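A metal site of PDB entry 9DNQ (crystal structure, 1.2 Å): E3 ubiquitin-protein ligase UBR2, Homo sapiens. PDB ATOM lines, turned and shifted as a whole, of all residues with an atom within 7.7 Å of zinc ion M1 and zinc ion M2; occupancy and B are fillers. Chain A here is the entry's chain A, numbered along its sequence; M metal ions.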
ATOM      1  N   LEU A   6     -10.835  25.055   0.038  1.00  0.00           N
ATOM      2  CA  LEU A   6     -10.144  24.329  -1.011  1.00  0.00           C
ATOM      3  C   LEU A   6     -10.891  23.049  -1.387  1.00  0.00           C
ATOM      4  O   LEU A   6     -10.981  22.718  -2.574  1.00  0.00           O
ATOM      5  CB  LEU A   6      -8.721  24.021  -0.568  1.00  0.00           C
ATOM      6  CG  LEU A   6      -7.823  23.273  -1.535  1.00  0.00           C
ATOM      7  CD1 LEU A   6      -7.746  23.982  -2.876  1.00  0.00           C
ATOM      8  CD2 LEU A   6      -6.436  23.148  -0.914  1.00  0.00           C
ATOM      9  N   CYS A   7     -11.427  22.326  -0.412  1.00  0.00           N
ATOM     10  CA  CYS A   7     -12.056  21.042  -0.731  1.00  0.00           C
ATOM     11  C   CYS A   7     -13.451  21.222  -1.320  1.00  0.00           C
ATOM     12  O   CYS A   7     -13.741  20.766  -2.433  1.00  0.00           O
ATOM     13  CB  CYS A   7     -12.037  20.102   0.471  1.00  0.00           C
ATOM     14  SG  CYS A   7     -13.045  18.628   0.218  1.00  0.00           S
ATOM     15  N   GLY A   8     -14.333  21.904  -0.601  1.00  0.00           N
ATOM     16  CA  GLY A   8     -15.679  22.194  -1.058  1.00  0.00           C
ATOM     17  C   GLY A   8     -16.757  21.294  -0.498  1.00  0.00           C
ATOM     18  O   GLY A   8     -17.935  21.627  -0.604  1.00  0.00           O
ATOM     19  N   ARG A   9     -16.376  20.180   0.131  1.00  0.00           N
ATOM     20  CA  ARG A   9     -17.352  19.216   0.614  1.00  0.00           C
ATOM     21  C   ARG A   9     -18.149  19.770   1.795  1.00  0.00           C
ATOM     22  O   ARG A   9     -17.572  20.324   2.744  1.00  0.00           O
ATOM     23  CB  ARG A   9     -16.680  17.913   1.022  1.00  0.00           C
ATOM     24  CG  ARG A   9     -16.166  17.069  -0.135  1.00  0.00           C
ATOM     25  CD  ARG A   9     -17.293  16.582  -1.089  1.00  0.00           C
ATOM     26  NE  ARG A   9     -18.580  16.383  -0.414  1.00  0.00           N
ATOM     27  CZ  ARG A   9     -18.832  15.402   0.436  1.00  0.00           C
ATOM     28  NH1 ARG A   9     -17.941  14.461   0.707  1.00  0.00           N
ATOM     29  NH2 ARG A   9     -20.022  15.372   1.056  1.00  0.00           N
ATOM     30  N   VAL A  10     -19.456  19.578   1.736  1.00  0.00           N
ATOM     31  CA  VAL A  10     -20.380  19.810   2.831  1.00  0.00           C
ATOM     32  C   VAL A  10     -20.923  18.438   3.215  1.00  0.00           C
ATOM     33  O   VAL A  10     -21.345  17.668   2.347  1.00  0.00           O
ATOM     34  CB  VAL A  10     -21.534  20.732   2.395  1.00  0.00           C
ATOM     35  CG1 VAL A  10     -22.597  20.824   3.477  1.00  0.00           C
ATOM     36  CG2 VAL A  10     -21.000  22.109   2.048  1.00  0.00           C
ATOM     37  N   PHE A  11     -20.918  18.117   4.498  1.00  0.00           N
ATOM     38  CA  PHE A  11     -21.189  16.743   4.888  1.00  0.00           C
ATOM     39  C   PHE A  11     -22.665  16.362   4.769  1.00  0.00           C
ATOM     40  O   PHE A  11     -23.567  17.113   5.155  1.00  0.00           O
ATOM     41  CB  PHE A  11     -20.684  16.447   6.301  1.00  0.00           C
ATOM     42  CG  PHE A  11     -19.200  16.622   6.435  1.00  0.00           C
ATOM     43  CD1 PHE A  11     -18.331  15.760   5.787  1.00  0.00           C
ATOM     44  CD2 PHE A  11     -18.664  17.680   7.150  1.00  0.00           C
ATOM     45  CE1 PHE A  11     -16.962  15.939   5.881  1.00  0.00           C
ATOM     46  CE2 PHE A  11     -17.304  17.859   7.239  1.00  0.00           C
ATOM     47  CZ  PHE A  11     -16.457  16.995   6.610  1.00  0.00           C
ATOM     48  N   VAL A  30     -12.047  19.364  10.805  1.00  0.00           N
ATOM     49  CA  VAL A  30     -12.354  18.039  10.283  1.00  0.00           C
ATOM     50  C   VAL A  30     -11.979  17.946   8.813  1.00  0.00           C
ATOM     51  O   VAL A  30     -11.900  18.949   8.086  1.00  0.00           O
ATOM     52  CB  VAL A  30     -13.847  17.653  10.439  1.00  0.00           C
ATOM     53  CG1 VAL A  30     -14.214  17.485  11.905  1.00  0.00           C
ATOM     54  CG2 VAL A  30     -14.767  18.647   9.709  1.00  0.00           C
ATOM     55  N   LEU A  31     -11.748  16.713   8.374  1.00  0.00           N
ATOM     56  CA  LEU A  31     -11.547  16.375   6.976  1.00  0.00           C
ATOM     57  C   LEU A  31     -12.609  15.381   6.538  1.00  0.00           C
ATOM     58  O   LEU A  31     -13.047  14.522   7.324  1.00  0.00           O
ATOM     59  CB  LEU A  31     -10.178  15.686   6.801  1.00  0.00           C
ATOM     60  CG  LEU A  31      -8.972  16.555   7.174  1.00  0.00           C
ATOM     61  CD1 LEU A  31      -7.694  15.725   7.060  1.00  0.00           C
ATOM     62  CD2 LEU A  31      -8.863  17.765   6.283  1.00  0.00           C
ATOM     63  N   CYS A  32     -13.015  15.491   5.283  1.00  0.00           N
ATOM     64  CA  CYS A  32     -13.808  14.424   4.675  1.00  0.00           C
ATOM     65  C   CYS A  32     -12.937  13.174   4.506  1.00  0.00           C
ATOM     66  O   CYS A  32     -11.714  13.203   4.638  1.00  0.00           O
ATOM     67  CB  CYS A  32     -14.368  14.851   3.313  1.00  0.00           C
ATOM     68  SG  CYS A  32     -13.122  15.069   1.957  1.00  0.00           S
ATOM     69  N   MET A  33     -13.612  12.048   4.261  1.00  0.00           N
ATOM     70  CA  MET A  33     -12.902  10.770   4.277  1.00  0.00           C
ATOM     71  C   MET A  33     -11.800  10.722   3.205  1.00  0.00           C
ATOM     72  O   MET A  33     -10.686  10.259   3.469  1.00  0.00           O
ATOM     73  CB  MET A  33     -13.890   9.618   4.139  1.00  0.00           C
ATOM     74  CG  MET A  33     -13.212   8.259   4.172  1.00  0.00           C
ATOM     75  SD  MET A  33     -14.214   6.852   3.683  1.00  0.00           S
ATOM     76  CE  MET A  33     -13.934   6.950   1.928  1.00  0.00           C
ATOM     77  N   GLU A  34     -12.096  11.203   2.004  1.00  0.00           N
ATOM     78  CA  GLU A  34     -11.111  11.142   0.937  1.00  0.00           C
ATOM     79  C   GLU A  34      -9.901  11.999   1.263  1.00  0.00           C
ATOM     80  O   GLU A  34      -8.750  11.578   1.055  1.00  0.00           O
ATOM     81  CB  GLU A  34     -11.784  11.554  -0.368  1.00  0.00           C
ATOM     82  CG  GLU A  34     -12.736  10.470  -0.896  1.00  0.00           C
ATOM     83  CD  GLU A  34     -14.136  10.407  -0.227  1.00  0.00           C
ATOM     84  OE1 GLU A  34     -14.531  11.254   0.639  1.00  0.00           O
ATOM     85  OE2 GLU A  34     -14.889   9.467  -0.585  1.00  0.00           O
ATOM     86  N   CYS A  35     -10.127  13.199   1.817  1.00  0.00           N
ATOM     87  CA  CYS A  35      -9.011  14.033   2.250  1.00  0.00           C
ATOM     88  C   CYS A  35      -8.221  13.364   3.376  1.00  0.00           C
ATOM     89  O   CYS A  35      -6.994  13.302   3.325  1.00  0.00           O
ATOM     90  CB  CYS A  35      -9.518  15.425   2.642  1.00  0.00           C
ATOM     91  SG  CYS A  35     -10.041  16.414   1.232  1.00  0.00           S
ATOM     92  N   PHE A  36      -8.923  12.810   4.374  1.00  0.00           N
ATOM     93  CA  PHE A  36      -8.263  12.191   5.528  1.00  0.00           C
ATOM     94  C   PHE A  36      -7.388  11.030   5.083  1.00  0.00           C
ATOM     95  O   PHE A  36      -6.223  10.897   5.488  1.00  0.00           O
ATOM     96  CB  PHE A  36      -9.331  11.705   6.519  1.00  0.00           C
ATOM     97  CG  PHE A  36      -8.779  10.912   7.666  1.00  0.00           C
ATOM     98  CD1 PHE A  36      -8.052  11.528   8.670  1.00  0.00           C
ATOM     99  CD2 PHE A  36      -8.948   9.535   7.715  1.00  0.00           C
ATOM    100  CE1 PHE A  36      -7.523  10.773   9.716  1.00  0.00           C
ATOM    101  CE2 PHE A  36      -8.433   8.800   8.762  1.00  0.00           C
ATOM    102  CZ  PHE A  36      -7.723   9.416   9.757  1.00  0.00           C
ATOM    103  N   GLY A  38      -5.987  10.342   2.314  1.00  0.00           N
ATOM    104  CA  GLY A  38      -4.841  10.787   1.552  1.00  0.00           C
ATOM    105  C   GLY A  38      -3.986  11.824   2.274  1.00  0.00           C
ATOM    106  O   GLY A  38      -3.223  12.564   1.648  1.00  0.00           O
ATOM    107  N   SER A  39      -4.072  11.844   3.602  1.00  0.00           N
ATOM    108  CA  SER A  39      -3.355  12.828   4.406  1.00  0.00           C
ATOM    109  C   SER A  39      -2.405  12.131   5.376  1.00  0.00           C
ATOM    110  O   SER A  39      -2.536  10.945   5.655  1.00  0.00           O
ATOM    111  CB  SER A  39      -4.338  13.701   5.194  1.00  0.00           C
ATOM    112  OG  SER A  39      -4.732  13.060   6.401  1.00  0.00           O
ATOM    113  N   PHE A  56     -18.412  21.265   7.091  1.00  0.00           N
ATOM    114  CA  PHE A  56     -17.644  21.258   5.857  1.00  0.00           C
ATOM    115  C   PHE A  56     -16.188  20.867   6.124  1.00  0.00           C
ATOM    116  O   PHE A  56     -15.670  21.008   7.232  1.00  0.00           O
ATOM    117  CB  PHE A  56     -17.697  22.609   5.127  1.00  0.00           C
ATOM    118  CG  PHE A  56     -17.190  23.776   5.930  1.00  0.00           C
ATOM    119  CD1 PHE A  56     -17.967  24.367   6.913  1.00  0.00           C
ATOM    120  CD2 PHE A  56     -15.937  24.311   5.665  1.00  0.00           C
ATOM    121  CE1 PHE A  56     -17.496  25.449   7.641  1.00  0.00           C
ATOM    122  CE2 PHE A  56     -15.467  25.408   6.394  1.00  0.00           C
ATOM    123  CZ  PHE A  56     -16.258  25.970   7.383  1.00  0.00           C
ATOM    124  N   CYS A  57     -15.549  20.350   5.076  1.00  0.00           N
ATOM    125  CA  CYS A  57     -14.175  19.879   5.146  1.00  0.00           C
ATOM    126  C   CYS A  57     -13.190  21.054   5.227  1.00  0.00           C
ATOM    127  O   CYS A  57     -13.301  22.022   4.472  1.00  0.00           O
ATOM    128  CB  CYS A  57     -13.865  19.014   3.922  1.00  0.00           C
ATOM    129  SG  CYS A  57     -12.159  18.407   3.877  1.00  0.00           S
ATOM    130  N   ASP A  58     -12.222  20.933   6.141  1.00  0.00           N
ATOM    131  CA  ASP A  58     -11.213  21.961   6.388  1.00  0.00           C
ATOM    132  C   ASP A  58      -9.875  21.638   5.724  1.00  0.00           C
ATOM    133  O   ASP A  58      -8.837  22.185   6.143  1.00  0.00           O
ATOM    134  CB  ASP A  58     -11.013  22.121   7.895  1.00  0.00           C
ATOM    135  CG  ASP A  58     -12.257  22.581   8.613  1.00  0.00           C
ATOM    136  OD1 ASP A  58     -12.789  23.656   8.230  1.00  0.00           O
ATOM    137  OD2 ASP A  58     -12.709  21.878   9.540  1.00  0.00           O
ATOM    138  N   CYS A  59      -9.856  20.780   4.709  1.00  0.00           N
ATOM    139  CA  CYS A  59      -8.603  20.519   4.009  1.00  0.00           C
ATOM    140  C   CYS A  59      -8.041  21.814   3.452  1.00  0.00           C
ATOM    141  O   CYS A  59      -8.782  22.645   2.902  1.00  0.00           O
ATOM    142  CB  CYS A  59      -8.789  19.508   2.877  1.00  0.00           C
ATOM    143  SG  CYS A  59      -7.242  18.925   2.199  1.00  0.00           S
ATOM    144  N   GLY A  60      -6.729  22.009   3.605  1.00  0.00           N
ATOM    145  CA  GLY A  60      -6.092  23.193   3.083  1.00  0.00           C
ATOM    146  C   GLY A  60      -6.227  24.420   3.942  1.00  0.00           C
ATOM    147  O   GLY A  60      -5.696  25.472   3.572  1.00  0.00           O
ATOM    148  N   PRO A  69      -1.383  20.464   6.303  1.00  0.00           N
ATOM    149  CA  PRO A  69      -2.674  21.086   5.940  1.00  0.00           C
ATOM    150  C   PRO A  69      -3.303  20.571   4.656  1.00  0.00           C
ATOM    151  O   PRO A  69      -4.521  20.727   4.507  1.00  0.00           O
ATOM    152  CB  PRO A  69      -2.325  22.580   5.813  1.00  0.00           C
ATOM    153  CG  PRO A  69      -0.878  22.569   5.450  1.00  0.00           C
ATOM    154  CD  PRO A  69      -0.286  21.451   6.256  1.00  0.00           C
ATOM    155  N   TYR A  70      -2.546  20.005   3.728  1.00  0.00           N
ATOM    156  CA  TYR A  70      -3.056  19.603   2.412  1.00  0.00           C
ATOM    157  C   TYR A  70      -2.952  18.092   2.249  1.00  0.00           C
ATOM    158  O   TYR A  70      -1.883  17.517   2.433  1.00  0.00           O
ATOM    159  CB  TYR A  70      -2.257  20.252   1.280  1.00  0.00           C
ATOM    160  CG  TYR A  70      -2.195  21.755   1.333  1.00  0.00           C
ATOM    161  CD1 TYR A  70      -3.317  22.521   1.092  1.00  0.00           C
ATOM    162  CD2 TYR A  70      -1.008  22.398   1.648  1.00  0.00           C
ATOM    163  CE1 TYR A  70      -3.254  23.909   1.170  1.00  0.00           C
ATOM    164  CE2 TYR A  70      -0.939  23.787   1.714  1.00  0.00           C
ATOM    165  CZ  TYR A  70      -2.058  24.539   1.489  1.00  0.00           C
ATOM    166  OH  TYR A  70      -1.950  25.908   1.568  1.00  0.00           O
ATOM    167  N   CYS A  71      -4.065  17.469   1.864  1.00  0.00           N
ATOM    168  CA  CYS A  71      -4.022  16.062   1.478  1.00  0.00           C
ATOM    169  C   CYS A  71      -3.438  15.941   0.067  1.00  0.00           C
ATOM    170  O   CYS A  71      -3.186  16.929  -0.620  1.00  0.00           O
ATOM    171  CB  CYS A  71      -5.414  15.438   1.504  1.00  0.00           C
ATOM    172  SG  CYS A  71      -6.440  15.860   0.073  1.00  0.00           S
ATOM    173  N   GLN A  72      -3.236  14.700  -0.382  1.00  0.00           N
ATOM    174  CA  GLN A  72      -2.576  14.527  -1.663  1.00  0.00           C
ATOM    175  C   GLN A  72      -3.443  15.009  -2.829  1.00  0.00           C
ATOM    176  O   GLN A  72      -2.919  15.568  -3.798  1.00  0.00           O
ATOM    177  CB  GLN A  72      -2.085  13.082  -1.823  1.00  0.00           C
ATOM    178  CG  GLN A  72      -1.110  12.869  -2.987  1.00  0.00           C
ATOM    179  CD  GLN A  72       0.240  12.288  -2.507  1.00  0.00           C
ATOM    180  OE1 GLN A  72       0.291  11.197  -1.924  1.00  0.00           O
ATOM    181  NE2 GLN A  72       1.330  13.013  -2.754  1.00  0.00           N
ATOM    182  N   LYS A  73      -4.758  14.861  -2.736  1.00  0.00           N
ATOM    183  CA  LYS A  73      -5.600  15.369  -3.805  1.00  0.00           C
ATOM    184  C   LYS A  73      -5.525  16.899  -3.897  1.00  0.00           C
ATOM    185  O   LYS A  73      -5.606  17.464  -4.995  1.00  0.00           O
ATOM    186  CB  LYS A  73      -7.032  14.883  -3.572  1.00  0.00           C
ATOM    187  CG  LYS A  73      -8.088  15.523  -4.451  1.00  0.00           C
ATOM    188  CD  LYS A  73      -9.453  14.977  -4.071  1.00  0.00           C
ATOM    189  CE  LYS A  73     -10.472  15.195  -5.161  1.00  0.00           C
ATOM    190  NZ  LYS A  73     -11.115  16.528  -5.054  1.00  0.00           N
ATOM    191  N   HIS A  74      -5.358  17.562  -2.757  1.00  0.00           N
ATOM    192  CA  HIS A  74      -5.316  19.020  -2.686  1.00  0.00           C
ATOM    193  C   HIS A  74      -3.893  19.553  -2.522  1.00  0.00           C
ATOM    194  O   HIS A  74      -3.711  20.684  -2.076  1.00  0.00           O
ATOM    195  CB  HIS A  74      -6.275  19.499  -1.601  1.00  0.00           C
ATOM    196  CG  HIS A  74      -7.706  19.206  -1.925  1.00  0.00           C
ATOM    197  ND1 HIS A  74      -8.496  18.367  -1.166  1.00  0.00           N
ATOM    198  CD2 HIS A  74      -8.467  19.604  -2.971  1.00  0.00           C
ATOM    199  CE1 HIS A  74      -9.690  18.279  -1.733  1.00  0.00           C
ATOM    200  NE2 HIS A  74      -9.701  19.024  -2.820  1.00  0.00           N
ATOM    201  N   GLU A  75      -2.891  18.765  -2.919  1.00  0.00           N
ATOM    202  CA  GLU A  75      -1.495  19.174  -2.721  1.00  0.00           C
ATOM    203  C   GLU A  75      -1.142  20.407  -3.555  1.00  0.00           C
ATOM    204  O   GLU A  75      -0.151  21.055  -3.220  1.00  0.00           O
ATOM    205  CB  GLU A  75      -0.511  18.048  -3.013  1.00  0.00           C
ATOM    206  CG  GLU A  75      -0.402  17.715  -4.470  1.00  0.00           C
ATOM    207  CD  GLU A  75       0.486  16.519  -4.732  1.00  0.00           C
ATOM    208  OE1 GLU A  75       0.895  15.847  -3.764  1.00  0.00           O
ATOM    209  OE2 GLU A  75       0.753  16.247  -5.924  1.00  0.00           O
ATOM    210  OXT GLU A  75      -1.809  20.757  -4.543  1.00  0.00           O
HETATM  211 ZN    ZN M   1     -12.218  17.224   1.878  1.00  0.00          ZN
HETATM  212 ZN    ZN M   2      -8.009  17.467   0.628  1.00  0.00          ZN
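The backbone NH (N) of Cys 59 sits close to the side-chain sulfur (SG) of Cys 57, at 3.4 Å.
SG of Cys 71 lies close to N of Lys 73, at 3.4 Å.
The backbone NH (N) of Arg 9 sits close to the side-chain sulfur (SG) of Cys 7 (3.7 Å).
N of Cys 57 is in hydrogen-bond range of O of Arg 9 (3.1 Å).
Four residues have an atom within 4 Å of zinc ion M1: Cys 7, Cys 32, Cys 35 and Cys 57.
Within 4 Å of zinc ion M2: Cys 35, Cys 59, Cys 71 and His 74.
The nearest printed residue that does not touch zinc ion M2 is Cys 7 (4.8 Å).
SG of Cys 57 is bound to zinc ion M1, at 2.3 Å.
SG of Cys 7 is bound to zinc ion M1, at 2.3 Å.
The side-chain sulfur (SG) of Cys 32 binds zinc ion M1 (2.3 Å).
Zinc ion M1 is bound by the side-chain sulfur (SG) of Cys 35.
Zinc ion M2 is bound by a ring nitrogen (ND1) of His 74 (2.1 Å), the side-chain sulfur (SG) of Cys 59 (2.3 Å), the side-chain sulfur (SG) of Cys 71 (2.3 Å) and the side-chain sulfur (SG) of Cys 35 (2.4 Å).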
